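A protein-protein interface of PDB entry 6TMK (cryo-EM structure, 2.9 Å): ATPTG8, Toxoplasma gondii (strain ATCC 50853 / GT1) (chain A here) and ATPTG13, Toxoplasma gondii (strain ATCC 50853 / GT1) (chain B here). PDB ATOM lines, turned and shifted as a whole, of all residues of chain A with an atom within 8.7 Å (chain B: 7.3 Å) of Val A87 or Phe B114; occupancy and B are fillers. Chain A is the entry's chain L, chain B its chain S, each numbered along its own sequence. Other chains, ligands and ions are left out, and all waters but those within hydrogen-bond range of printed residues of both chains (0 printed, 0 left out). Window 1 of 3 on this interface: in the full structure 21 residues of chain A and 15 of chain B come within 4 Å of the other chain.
NZ of Lys B116 lies within salt-bridge range of OD1 of Asp A83 (3.1 Å).
OE2 of Glu A100 is in hydrogen-bond range of NE2 of Gln B108, 3.0 Å away.
Of the printed residues of chain B, Asp A83 touches Phe B114 (3.7 Å) and Lys B116 (3.1 Å).
Printed residues of chain B within 4 Å of Val A87: Leu B105 (3.999 Å), Val B109 (3.9 Å) and Phe B114 (3.7 Å).
Printed residues of chain B within 4 Å of Asp A91: Gln B108 (3.7 Å).
Lys A111 touches none of the printed residues of chain B.
Gly B113 touches none of the printed residues of chain A.
Of the printed residues of chain A, Phe B114 touches Asp A83 (3.7 Å), Arg A86 (3.8 Å) and Val A87 (3.7 Å).
The nearest residue of chain A that does not touch Phe B114 is Thr A90 (5.5 Å).
Hydrophobic or aromatic side chains of chain A within 4 Å of the printed part of chain B: Ala A79 and Val A87.
Printed residues of chain B that touch a printed residue of chain A: Val B104, Leu B105, Gln B108, Val B109, Phe B114, Asp B115 and Lys B116.
Hydrophobic or aromatic side chains of chain B that line the printed part of chain A: Val B104, Leu B105, Val B109 and Phe B114.
Among the printed residues, 12 pairs touch across the chains.
Among the printed residues, Asp or Glu carboxylates within 4 Å of a Lys or Arg side-chain nitrogen of the other chain: Asp A83 with Lys B116.
The backbone carbonyl oxygen of Asn A78 sits at hydrogen-bond distance from the guanidinium group of Arg A86 (3.3 Å).
The side-chain hydroxyl (OG) of Ser A82 lies within hydrogen-bond range of the side-chain hydroxyl (OG) of Ser A84 (3.4 Å).
The backbone carbonyl oxygen (O) of Arg A86 lies within hydrogen-bond range of the side-chain hydroxyl (OG1) of Thr A90, 2.8 Å away.
The side-chain hydroxyl (OH) of Tyr A115 is in hydrogen-bond range of the side-chain carboxylate (OD2) of Asp A91, 3.2 Å away.
OE1 of Glu A100 is in salt-bridge range of NZ of Lys A111.
The side-chain carboxylate of Asp B115 is in hydrogen-bond range of the side-chain hydroxyl of Thr B117, 2.5 Å away.
Among the printed residues, merely in contact across the chains: Ala A79 with Lys B116 (3.3 Å), Val A87 with Phe B114 (3.7 Å), Asp A91 with Gln B108 (3.7 Å), Asp A83 with Phe B114 (3.7 Å), Arg A86 with Phe B114 (3.8 Å), Arg A86 with Asp B115 (3.8 Å), Ser A84 with Leu B105 (3.9 Å), Val A87 with Val B109 (3.9 Å), Glu A100 with Val B104 (3.9 Å) and Val A87 with Leu B105 (3.999 Å).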
ATOM      1  N   VAL A  76      -5.104 -25.991 -27.705  1.00  0.00           N
ATOM      2  CA  VAL A  76      -6.410 -26.517 -28.080  1.00  0.00           C
ATOM      3  C   VAL A  76      -6.613 -26.190 -29.557  1.00  0.00           C
ATOM      4  O   VAL A  76      -7.066 -25.102 -29.911  1.00  0.00           O
ATOM      5  CB  VAL A  76      -7.529 -25.941 -27.212  1.00  0.00           C
ATOM      6  CG1 VAL A  76      -8.818 -26.686 -27.465  1.00  0.00           C
ATOM      7  CG2 VAL A  76      -7.140 -26.004 -25.751  1.00  0.00           C
ATOM      8  N   ASN A  78      -8.302 -28.325 -31.968  1.00  0.00           N
ATOM      9  CA  ASN A  78      -9.198 -29.366 -32.445  1.00  0.00           C
ATOM     10  C   ASN A  78     -10.573 -28.761 -32.677  1.00  0.00           C
ATOM     11  O   ASN A  78     -11.144 -28.143 -31.774  1.00  0.00           O
ATOM     12  CB  ASN A  78      -9.275 -30.521 -31.450  1.00  0.00           C
ATOM     13  CG  ASN A  78     -10.019 -31.709 -32.001  1.00  0.00           C
ATOM     14  OD1 ASN A  78     -10.366 -31.747 -33.178  1.00  0.00           O
ATOM     15  ND2 ASN A  78     -10.253 -32.698 -31.156  1.00  0.00           N
ATOM     16  N   ALA A  79     -11.097 -28.943 -33.885  1.00  0.00           N
ATOM     17  CA  ALA A  79     -12.384 -28.382 -34.263  1.00  0.00           C
ATOM     18  C   ALA A  79     -13.544 -29.334 -34.024  1.00  0.00           C
ATOM     19  O   ALA A  79     -14.689 -28.879 -33.920  1.00  0.00           O
ATOM     20  CB  ALA A  79     -12.367 -27.977 -35.735  1.00  0.00           C
ATOM     21  N   LEU A  81     -14.251 -30.914 -31.397  1.00  0.00           N
ATOM     22  CA  LEU A  81     -14.626 -31.006 -29.997  1.00  0.00           C
ATOM     23  C   LEU A  81     -16.044 -30.507 -29.769  1.00  0.00           C
ATOM     24  O   LEU A  81     -16.547 -29.633 -30.481  1.00  0.00           O
ATOM     25  CB  LEU A  81     -13.674 -30.187 -29.132  1.00  0.00           C
ATOM     26  CG  LEU A  81     -12.366 -30.812 -28.677  1.00  0.00           C
ATOM     27  CD1 LEU A  81     -11.581 -29.800 -27.887  1.00  0.00           C
ATOM     28  CD2 LEU A  81     -12.646 -32.021 -27.845  1.00  0.00           C
ATOM     29  N   SER A  82     -16.689 -31.075 -28.757  1.00  0.00           N
ATOM     30  CA  SER A  82     -17.892 -30.481 -28.201  1.00  0.00           C
ATOM     31  C   SER A  82     -17.539 -29.194 -27.471  1.00  0.00           C
ATOM     32  O   SER A  82     -16.442 -29.041 -26.930  1.00  0.00           O
ATOM     33  CB  SER A  82     -18.578 -31.454 -27.251  1.00  0.00           C
ATOM     34  OG  SER A  82     -19.888 -31.023 -26.935  1.00  0.00           O
ATOM     35  N   ASP A  83     -18.484 -28.254 -27.461  1.00  0.00           N
ATOM     36  CA  ASP A  83     -18.242 -26.995 -26.768  1.00  0.00           C
ATOM     37  C   ASP A  83     -18.090 -27.213 -25.268  1.00  0.00           C
ATOM     38  O   ASP A  83     -17.283 -26.546 -24.614  1.00  0.00           O
ATOM     39  CB  ASP A  83     -19.372 -26.014 -27.063  1.00  0.00           C
ATOM     40  CG  ASP A  83     -19.203 -25.318 -28.396  1.00  0.00           C
ATOM     41  OD1 ASP A  83     -18.393 -25.794 -29.218  1.00  0.00           O
ATOM     42  OD2 ASP A  83     -19.879 -24.293 -28.624  1.00  0.00           O
ATOM     43  N   SER A  84     -18.841 -28.161 -24.708  1.00  0.00           N
ATOM     44  CA  SER A  84     -18.721 -28.455 -23.285  1.00  0.00           C
ATOM     45  C   SER A  84     -17.360 -29.058 -22.959  1.00  0.00           C
ATOM     46  O   SER A  84     -16.700 -28.650 -21.994  1.00  0.00           O
ATOM     47  CB  SER A  84     -19.846 -29.390 -22.856  1.00  0.00           C
ATOM     48  OG  SER A  84     -19.778 -30.621 -23.547  1.00  0.00           O
ATOM     49  N   GLN A  85     -16.932 -30.046 -23.746  1.00  0.00           N
ATOM     50  CA  GLN A  85     -15.607 -30.625 -23.554  1.00  0.00           C
ATOM     51  C   GLN A  85     -14.525 -29.569 -23.702  1.00  0.00           C
ATOM     52  O   GLN A  85     -13.539 -29.568 -22.957  1.00  0.00           O
ATOM     53  CB  GLN A  85     -15.387 -31.752 -24.555  1.00  0.00           C
ATOM     54  CG  GLN A  85     -15.945 -33.080 -24.131  1.00  0.00           C
ATOM     55  CD  GLN A  85     -15.873 -34.115 -25.232  1.00  0.00           C
ATOM     56  OE1 GLN A  85     -15.973 -33.789 -26.413  1.00  0.00           O
ATOM     57  NE2 GLN A  85     -15.702 -35.372 -24.850  1.00  0.00           N
ATOM     58  N   ARG A  86     -14.692 -28.662 -24.661  1.00  0.00           N
ATOM     59  CA  ARG A  86     -13.707 -27.614 -24.872  1.00  0.00           C
ATOM     60  C   ARG A  86     -13.646 -26.670 -23.683  1.00  0.00           C
ATOM     61  O   ARG A  86     -12.559 -26.275 -23.254  1.00  0.00           O
ATOM     62  CB  ARG A  86     -14.030 -26.848 -26.148  1.00  0.00           C
ATOM     63  CG  ARG A  86     -13.069 -25.737 -26.460  1.00  0.00           C
ATOM     64  CD  ARG A  86     -12.959 -25.503 -27.943  1.00  0.00           C
ATOM     65  NE  ARG A  86     -12.019 -24.432 -28.253  1.00  0.00           N
ATOM     66  CZ  ARG A  86     -11.385 -24.306 -29.411  1.00  0.00           C
ATOM     67  NH1 ARG A  86     -10.550 -23.297 -29.594  1.00  0.00           N
ATOM     68  NH2 ARG A  86     -11.581 -25.185 -30.381  1.00  0.00           N
ATOM     69  N   VAL A  87     -14.803 -26.297 -23.137  1.00  0.00           N
ATOM     70  CA  VAL A  87     -14.821 -25.450 -21.952  1.00  0.00           C
ATOM     71  C   VAL A  87     -14.128 -26.143 -20.791  1.00  0.00           C
ATOM     72  O   VAL A  87     -13.337 -25.530 -20.065  1.00  0.00           O
ATOM     73  CB  VAL A  87     -16.269 -25.078 -21.599  1.00  0.00           C
ATOM     74  CG1 VAL A  87     -16.341 -24.524 -20.206  1.00  0.00           C
ATOM     75  CG2 VAL A  87     -16.800 -24.081 -22.580  1.00  0.00           C
ATOM     76  N   MET A  88     -14.411 -27.429 -20.597  1.00  0.00           N
ATOM     77  CA  MET A  88     -13.814 -28.163 -19.487  1.00  0.00           C
ATOM     78  C   MET A  88     -12.296 -28.238 -19.631  1.00  0.00           C
ATOM     79  O   MET A  88     -11.548 -28.003 -18.672  1.00  0.00           O
ATOM     80  CB  MET A  88     -14.433 -29.553 -19.425  1.00  0.00           C
ATOM     81  CG  MET A  88     -14.387 -30.201 -18.067  1.00  0.00           C
ATOM     82  SD  MET A  88     -15.384 -31.690 -17.960  1.00  0.00           S
ATOM     83  CE  MET A  88     -16.736 -31.070 -16.976  1.00  0.00           C
ATOM     84  N   TRP A  89     -11.826 -28.560 -20.835  1.00  0.00           N
ATOM     85  CA  TRP A  89     -10.396 -28.668 -21.086  1.00  0.00           C
ATOM     86  C   TRP A  89      -9.701 -27.320 -20.950  1.00  0.00           C
ATOM     87  O   TRP A  89      -8.597 -27.236 -20.399  1.00  0.00           O
ATOM     88  CB  TRP A  89     -10.180 -29.268 -22.470  1.00  0.00           C
ATOM     89  CG  TRP A  89      -8.775 -29.602 -22.782  1.00  0.00           C
ATOM     90  CD1 TRP A  89      -8.031 -29.117 -23.806  1.00  0.00           C
ATOM     91  CD2 TRP A  89      -7.937 -30.505 -22.067  1.00  0.00           C
ATOM     92  NE1 TRP A  89      -6.778 -29.659 -23.776  1.00  0.00           N
ATOM     93  CE2 TRP A  89      -6.694 -30.518 -22.713  1.00  0.00           C
ATOM     94  CE3 TRP A  89      -8.115 -31.307 -20.941  1.00  0.00           C
ATOM     95  CZ2 TRP A  89      -5.639 -31.295 -22.273  1.00  0.00           C
ATOM     96  CZ3 TRP A  89      -7.069 -32.075 -20.511  1.00  0.00           C
ATOM     97  CH2 TRP A  89      -5.848 -32.065 -21.171  1.00  0.00           C
ATOM     98  N   THR A  90     -10.329 -26.253 -21.441  1.00  0.00           N
ATOM     99  CA  THR A  90      -9.738 -24.930 -21.322  1.00  0.00           C
ATOM    100  C   THR A  90      -9.733 -24.456 -19.878  1.00  0.00           C
ATOM    101  O   THR A  90      -8.860 -23.679 -19.489  1.00  0.00           O
ATOM    102  CB  THR A  90     -10.490 -23.945 -22.208  1.00  0.00           C
ATOM    103  OG1 THR A  90     -10.472 -24.417 -23.559  1.00  0.00           O
ATOM    104  CG2 THR A  90      -9.847 -22.587 -22.153  1.00  0.00           C
ATOM    105  N   ASP A  91     -10.690 -24.909 -19.070  1.00  0.00           N
ATOM    106  CA  ASP A  91     -10.625 -24.642 -17.640  1.00  0.00           C
ATOM    107  C   ASP A  91      -9.448 -25.367 -17.009  1.00  0.00           C
ATOM    108  O   ASP A  91      -8.724 -24.794 -16.187  1.00  0.00           O
ATOM    109  CB  ASP A  91     -11.930 -25.051 -16.966  1.00  0.00           C
ATOM    110  CG  ASP A  91     -13.063 -24.090 -17.254  1.00  0.00           C
ATOM    111  OD1 ASP A  91     -12.797 -22.992 -17.786  1.00  0.00           O
ATOM    112  OD2 ASP A  91     -14.222 -24.436 -16.946  1.00  0.00           O
ATOM    113  N   LEU A  92      -9.241 -26.631 -17.377  1.00  0.00           N
ATOM    114  CA  LEU A  92      -8.145 -27.388 -16.785  1.00  0.00           C
ATOM    115  C   LEU A  92      -6.782 -26.869 -17.228  1.00  0.00           C
ATOM    116  O   LEU A  92      -5.799 -27.029 -16.496  1.00  0.00           O
ATOM    117  CB  LEU A  92      -8.260 -28.864 -17.141  1.00  0.00           C
ATOM    118  CG  LEU A  92      -9.230 -29.709 -16.325  1.00  0.00           C
ATOM    119  CD1 LEU A  92      -9.422 -31.047 -16.979  1.00  0.00           C
ATOM    120  CD2 LEU A  92      -8.739 -29.898 -14.918  1.00  0.00           C
ATOM    121  N   VAL A  93      -6.693 -26.259 -18.405  1.00  0.00           N
ATOM    122  CA  VAL A  93      -5.416 -25.832 -18.961  1.00  0.00           C
ATOM    123  C   VAL A  93      -5.115 -24.374 -18.644  1.00  0.00           C
ATOM    124  O   VAL A  93      -3.978 -24.029 -18.328  1.00  0.00           O
ATOM    125  CB  VAL A  93      -5.396 -26.076 -20.485  1.00  0.00           C
ATOM    126  CG1 VAL A  93      -4.171 -25.447 -21.107  1.00  0.00           C
ATOM    127  CG2 VAL A  93      -5.428 -27.540 -20.787  1.00  0.00           C
ATOM    128  N   GLN A  94      -6.111 -23.507 -18.732  1.00  0.00           N
ATOM    129  CA  GLN A  94      -5.923 -22.066 -18.726  1.00  0.00           C
ATOM    130  C   GLN A  94      -6.614 -21.381 -17.563  1.00  0.00           C
ATOM    131  O   GLN A  94      -6.069 -20.427 -17.003  1.00  0.00           O
ATOM    132  CB  GLN A  94      -6.446 -21.479 -20.042  1.00  0.00           C
ATOM    133  CG  GLN A  94      -5.774 -20.203 -20.479  1.00  0.00           C
ATOM    134  CD  GLN A  94      -6.241 -19.749 -21.846  1.00  0.00           C
ATOM    135  OE1 GLN A  94      -7.098 -20.383 -22.461  1.00  0.00           O
ATOM    136  NE2 GLN A  94      -5.685 -18.645 -22.327  1.00  0.00           N
ATOM    137  N   GLY A  95      -7.808 -21.840 -17.186  1.00  0.00           N
ATOM    138  CA  GLY A  95      -8.606 -21.203 -16.176  1.00  0.00           C
ATOM    139  C   GLY A  95      -8.650 -21.975 -14.875  1.00  0.00           C
ATOM    140  O   GLY A  95      -7.763 -22.781 -14.561  1.00  0.00           O
ATOM    141  N   LYS A  96      -9.704 -21.725 -14.103  1.00  0.00           N
ATOM    142  CA  LYS A  96      -9.884 -22.314 -12.785  1.00  0.00           C
ATOM    143  C   LYS A  96     -11.076 -23.256 -12.791  1.00  0.00           C
ATOM    144  O   LYS A  96     -12.205 -22.801 -13.022  1.00  0.00           O
ATOM    145  CB  LYS A  96     -10.084 -21.225 -11.739  1.00  0.00           C
ATOM    146  CG  LYS A  96     -10.119 -21.740 -10.328  1.00  0.00           C
ATOM    147  CD  LYS A  96      -9.849 -20.637  -9.336  1.00  0.00           C
ATOM    148  CE  LYS A  96     -10.019 -21.121  -7.914  1.00  0.00           C
ATOM    149  NZ  LYS A  96      -9.076 -20.452  -6.985  1.00  0.00           N
ATOM    150  N   PRO A  97     -10.896 -24.553 -12.549  1.00  0.00           N
ATOM    151  CA  PRO A  97     -12.062 -25.430 -12.396  1.00  0.00           C
ATOM    152  C   PRO A  97     -12.779 -25.151 -11.084  1.00  0.00           C
ATOM    153  O   PRO A  97     -12.171 -25.166 -10.013  1.00  0.00           O
ATOM    154  CB  PRO A  97     -11.457 -26.839 -12.418  1.00  0.00           C
ATOM    155  CG  PRO A  97     -10.067 -26.674 -12.898  1.00  0.00           C
ATOM    156  CD  PRO A  97      -9.641 -25.314 -12.506  1.00  0.00           C
ATOM    157  N   GLU A 100     -20.344 -24.224  -9.799  1.00  0.00           N
ATOM    158  CA  GLU A 100     -21.167 -23.036  -9.661  1.00  0.00           C
ATOM    159  C   GLU A 100     -22.229 -23.243  -8.592  1.00  0.00           C
ATOM    160  O   GLU A 100     -22.685 -24.363  -8.348  1.00  0.00           O
ATOM    161  CB  GLU A 100     -21.828 -22.689 -10.992  1.00  0.00           C
ATOM    162  CG  GLU A 100     -20.870 -22.120 -12.013  1.00  0.00           C
ATOM    163  CD  GLU A 100     -20.044 -23.192 -12.686  1.00  0.00           C
ATOM    164  OE1 GLU A 100     -19.992 -24.318 -12.153  1.00  0.00           O
ATOM    165  OE2 GLU A 100     -19.445 -22.911 -13.745  1.00  0.00           O
ATOM    166  N   LYS A 111     -20.141 -32.898 -11.943  1.00  0.00           N
ATOM    167  CA  LYS A 111     -19.139 -32.066 -12.596  1.00  0.00           C
ATOM    168  C   LYS A 111     -17.741 -32.397 -12.101  1.00  0.00           C
ATOM    169  O   LYS A 111     -16.796 -32.497 -12.894  1.00  0.00           O
ATOM    170  CB  LYS A 111     -19.450 -30.593 -12.350  1.00  0.00           C
ATOM    171  CG  LYS A 111     -18.801 -29.644 -13.322  1.00  0.00           C
ATOM    172  CD  LYS A 111     -19.157 -28.217 -13.017  1.00  0.00           C
ATOM    173  CE  LYS A 111     -18.375 -27.261 -13.883  1.00  0.00           C
ATOM    174  NZ  LYS A 111     -18.829 -25.855 -13.738  1.00  0.00           N
ATOM    175  N   TYR A 115     -14.549 -33.831 -14.226  1.00  0.00           N
ATOM    176  CA  TYR A 115     -13.216 -33.244 -14.175  1.00  0.00           C
ATOM    177  C   TYR A 115     -12.172 -34.290 -13.823  1.00  0.00           C
ATOM    178  O   TYR A 115     -11.123 -34.380 -14.468  1.00  0.00           O
ATOM    179  CB  TYR A 115     -13.175 -32.098 -13.165  1.00  0.00           C
ATOM    180  CG  TYR A 115     -13.583 -30.751 -13.700  1.00  0.00           C
ATOM    181  CD1 TYR A 115     -12.924 -30.179 -14.769  1.00  0.00           C
ATOM    182  CD2 TYR A 115     -14.606 -30.035 -13.109  1.00  0.00           C
ATOM    183  CE1 TYR A 115     -13.284 -28.946 -15.248  1.00  0.00           C
ATOM    184  CE2 TYR A 115     -14.975 -28.801 -13.584  1.00  0.00           C
ATOM    185  CZ  TYR A 115     -14.310 -28.259 -14.654  1.00  0.00           C
ATOM    186  OH  TYR A 115     -14.671 -27.022 -15.139  1.00  0.00           O
ATOM    187  N   LEU A 118     -11.677 -36.931 -16.729  1.00  0.00           N
ATOM    188  CA  LEU A 118     -10.946 -36.317 -17.828  1.00  0.00           C
ATOM    189  C   LEU A 118      -9.479 -36.121 -17.472  1.00  0.00           C
ATOM    190  O   LEU A 118      -8.585 -36.504 -18.237  1.00  0.00           O
ATOM    191  CB  LEU A 118     -11.612 -34.988 -18.180  1.00  0.00           C
ATOM    192  CG  LEU A 118     -10.895 -34.006 -19.092  1.00  0.00           C
ATOM    193  CD1 LEU A 118     -10.366 -34.713 -20.296  1.00  0.00           C
ATOM    194  CD2 LEU A 118     -11.851 -32.908 -19.496  1.00  0.00           C
ATOM    195  N   VAL B 104     -25.157 -25.562 -17.828  1.00  0.00           N
ATOM    196  CA  VAL B 104     -24.380 -24.550 -17.122  1.00  0.00           C
ATOM    197  C   VAL B 104     -23.095 -24.231 -17.875  1.00  0.00           C
ATOM    198  O   VAL B 104     -22.651 -23.077 -17.911  1.00  0.00           O
ATOM    199  CB  VAL B 104     -24.091 -25.001 -15.682  1.00  0.00           C
ATOM    200  CG1 VAL B 104     -22.943 -24.213 -15.107  1.00  0.00           C
ATOM    201  CG2 VAL B 104     -25.318 -24.814 -14.828  1.00  0.00           C
ATOM    202  N   LEU B 105     -22.470 -25.241 -18.481  1.00  0.00           N
ATOM    203  CA  LEU B 105     -21.201 -25.015 -19.166  1.00  0.00           C
ATOM    204  C   LEU B 105     -21.377 -24.134 -20.393  1.00  0.00           C
ATOM    205  O   LEU B 105     -20.509 -23.312 -20.703  1.00  0.00           O
ATOM    206  CB  LEU B 105     -20.572 -26.341 -19.578  1.00  0.00           C
ATOM    207  CG  LEU B 105     -19.953 -27.223 -18.500  1.00  0.00           C
ATOM    208  CD1 LEU B 105     -19.448 -28.490 -19.131  1.00  0.00           C
ATOM    209  CD2 LEU B 105     -18.830 -26.516 -17.791  1.00  0.00           C
ATOM    210  N   LEU B 106     -22.491 -24.294 -21.105  1.00  0.00           N
ATOM    211  CA  LEU B 106     -22.704 -23.522 -22.322  1.00  0.00           C
ATOM    212  C   LEU B 106     -22.828 -22.028 -22.056  1.00  0.00           C
ATOM    213  O   LEU B 106     -22.740 -21.235 -22.998  1.00  0.00           O
ATOM    214  CB  LEU B 106     -23.951 -24.015 -23.045  1.00  0.00           C
ATOM    215  CG  LEU B 106     -23.878 -25.427 -23.626  1.00  0.00           C
ATOM    216  CD1 LEU B 106     -25.204 -25.798 -24.244  1.00  0.00           C
ATOM    217  CD2 LEU B 106     -22.763 -25.560 -24.634  1.00  0.00           C
ATOM    218  N   GLU B 107     -23.040 -21.627 -20.803  1.00  0.00           N
ATOM    219  CA  GLU B 107     -23.044 -20.207 -20.474  1.00  0.00           C
ATOM    220  C   GLU B 107     -21.644 -19.608 -20.519  1.00  0.00           C
ATOM    221  O   GLU B 107     -21.493 -18.411 -20.782  1.00  0.00           O
ATOM    222  CB  GLU B 107     -23.660 -19.994 -19.095  1.00  0.00           C
ATOM    223  CG  GLU B 107     -25.149 -20.265 -19.038  1.00  0.00           C
ATOM    224  CD  GLU B 107     -25.643 -20.512 -17.628  1.00  0.00           C
ATOM    225  OE1 GLU B 107     -25.017 -19.997 -16.677  1.00  0.00           O
ATOM    226  OE2 GLU B 107     -26.660 -21.219 -17.469  1.00  0.00           O
ATOM    227  N   GLN B 108     -20.615 -20.414 -20.267  1.00  0.00           N
ATOM    228  CA  GLN B 108     -19.241 -19.935 -20.297  1.00  0.00           C
ATOM    229  C   GLN B 108     -18.683 -19.790 -21.703  1.00  0.00           C
ATOM    230  O   GLN B 108     -17.583 -19.250 -21.862  1.00  0.00           O
ATOM    231  CB  GLN B 108     -18.347 -20.882 -19.504  1.00  0.00           C
ATOM    232  CG  GLN B 108     -18.759 -21.048 -18.065  1.00  0.00           C
ATOM    233  CD  GLN B 108     -17.742 -21.811 -17.258  1.00  0.00           C
ATOM    234  OE1 GLN B 108     -16.539 -21.577 -17.367  1.00  0.00           O
ATOM    235  NE2 GLN B 108     -18.218 -22.735 -16.440  1.00  0.00           N
ATOM    236  N   VAL B 109     -19.393 -20.260 -22.717  1.00  0.00           N
ATOM    237  CA  VAL B 109     -18.917 -20.089 -24.092  1.00  0.00           C
ATOM    238  C   VAL B 109     -18.989 -18.613 -24.466  1.00  0.00           C
ATOM    239  O   VAL B 109     -20.026 -17.968 -24.225  1.00  0.00           O
ATOM    240  CB  VAL B 109     -19.743 -20.943 -25.048  1.00  0.00           C
ATOM    241  CG1 VAL B 109     -19.351 -20.665 -26.481  1.00  0.00           C
ATOM    242  CG2 VAL B 109     -19.557 -22.404 -24.731  1.00  0.00           C
ATOM    243  N   PRO B 110     -17.941 -18.034 -25.046  1.00  0.00           N
ATOM    244  CA  PRO B 110     -17.984 -16.610 -25.385  1.00  0.00           C
ATOM    245  C   PRO B 110     -19.026 -16.315 -26.451  1.00  0.00           C
ATOM    246  O   PRO B 110     -19.496 -17.199 -27.169  1.00  0.00           O
ATOM    247  CB  PRO B 110     -16.569 -16.326 -25.899  1.00  0.00           C
ATOM    248  CG  PRO B 110     -16.081 -17.647 -26.363  1.00  0.00           C
ATOM    249  CD  PRO B 110     -16.633 -18.618 -25.378  1.00  0.00           C
ATOM    250  N   ALA B 111     -19.387 -15.038 -26.541  1.00  0.00           N
ATOM    251  CA  ALA B 111     -20.328 -14.601 -27.562  1.00  0.00           C
ATOM    252  C   ALA B 111     -19.753 -14.840 -28.950  1.00  0.00           C
ATOM    253  O   ALA B 111     -18.607 -14.478 -29.235  1.00  0.00           O
ATOM    254  CB  ALA B 111     -20.660 -13.124 -27.371  1.00  0.00           C
ATOM    255  N   GLY B 112     -20.555 -15.455 -29.815  1.00  0.00           N
ATOM    256  CA  GLY B 112     -20.105 -15.867 -31.125  1.00  0.00           C
ATOM    257  C   GLY B 112     -19.472 -17.238 -31.175  1.00  0.00           C
ATOM    258  O   GLY B 112     -19.073 -17.678 -32.262  1.00  0.00           O
ATOM    259  N   GLY B 113     -19.363 -17.924 -30.045  1.00  0.00           N
ATOM    260  CA  GLY B 113     -18.811 -19.257 -30.028  1.00  0.00           C
ATOM    261  C   GLY B 113     -17.296 -19.255 -30.072  1.00  0.00           C
ATOM    262  O   GLY B 113     -16.626 -18.237 -29.884  1.00  0.00           O
ATOM    263  N   PHE B 114     -16.753 -20.441 -30.327  1.00  0.00           N
ATOM    264  CA  PHE B 114     -15.315 -20.637 -30.376  1.00  0.00           C
ATOM    265  C   PHE B 114     -14.790 -20.438 -31.790  1.00  0.00           C
ATOM    266  O   PHE B 114     -15.455 -20.767 -32.776  1.00  0.00           O
ATOM    267  CB  PHE B 114     -14.935 -22.034 -29.888  1.00  0.00           C
ATOM    268  CG  PHE B 114     -15.143 -22.245 -28.422  1.00  0.00           C
ATOM    269  CD1 PHE B 114     -14.361 -21.579 -27.503  1.00  0.00           C
ATOM    270  CD2 PHE B 114     -16.103 -23.122 -27.964  1.00  0.00           C
ATOM    271  CE1 PHE B 114     -14.543 -21.774 -26.155  1.00  0.00           C
ATOM    272  CE2 PHE B 114     -16.286 -23.319 -26.618  1.00  0.00           C
ATOM    273  CZ  PHE B 114     -15.502 -22.645 -25.713  1.00  0.00           C
ATOM    274  N   ASP B 115     -13.583 -19.887 -31.878  1.00  0.00           N
ATOM    275  CA  ASP B 115     -12.847 -19.822 -33.138  1.00  0.00           C
ATOM    276  C   ASP B 115     -12.208 -21.187 -33.356  1.00  0.00           C
ATOM    277  O   ASP B 115     -11.088 -21.455 -32.919  1.00  0.00           O
ATOM    278  CB  ASP B 115     -11.809 -18.708 -33.104  1.00  0.00           C
ATOM    279  CG  ASP B 115     -11.326 -18.320 -34.486  1.00  0.00           C
ATOM    280  OD1 ASP B 115     -10.967 -17.141 -34.683  1.00  0.00           O
ATOM    281  OD2 ASP B 115     -11.310 -19.194 -35.377  1.00  0.00           O
ATOM    282  N   LYS B 116     -12.939 -22.064 -34.038  1.00  0.00           N
ATOM    283  CA  LYS B 116     -12.474 -23.418 -34.302  1.00  0.00           C
ATOM    284  C   LYS B 116     -11.410 -23.483 -35.387  1.00  0.00           C
ATOM    285  O   LYS B 116     -10.894 -24.572 -35.660  1.00  0.00           O
ATOM    286  CB  LYS B 116     -13.657 -24.302 -34.693  1.00  0.00           C
ATOM    287  CG  LYS B 116     -14.546 -24.678 -33.529  1.00  0.00           C
ATOM    288  CD  LYS B 116     -15.569 -25.721 -33.925  1.00  0.00           C
ATOM    289  CE  LYS B 116     -16.257 -26.301 -32.708  1.00  0.00           C
ATOM    290  NZ  LYS B 116     -16.913 -25.249 -31.890  1.00  0.00           N
ATOM    291  N   THR B 117     -11.072 -22.356 -36.012  1.00  0.00           N
ATOM    292  CA  THR B 117     -10.049 -22.363 -37.049  1.00  0.00           C
ATOM    293  C   THR B 117      -8.654 -22.327 -36.443  1.00  0.00           C
ATOM    294  O   THR B 117      -7.742 -23.003 -36.931  1.00  0.00           O
ATOM    295  CB  THR B 117     -10.243 -21.176 -37.993  1.00  0.00           C
ATOM    296  OG1 THR B 117      -9.895 -19.963 -37.316  1.00  0.00           O
ATOM    297  CG2 THR B 117     -11.685 -21.098 -38.460  1.00  0.00           C
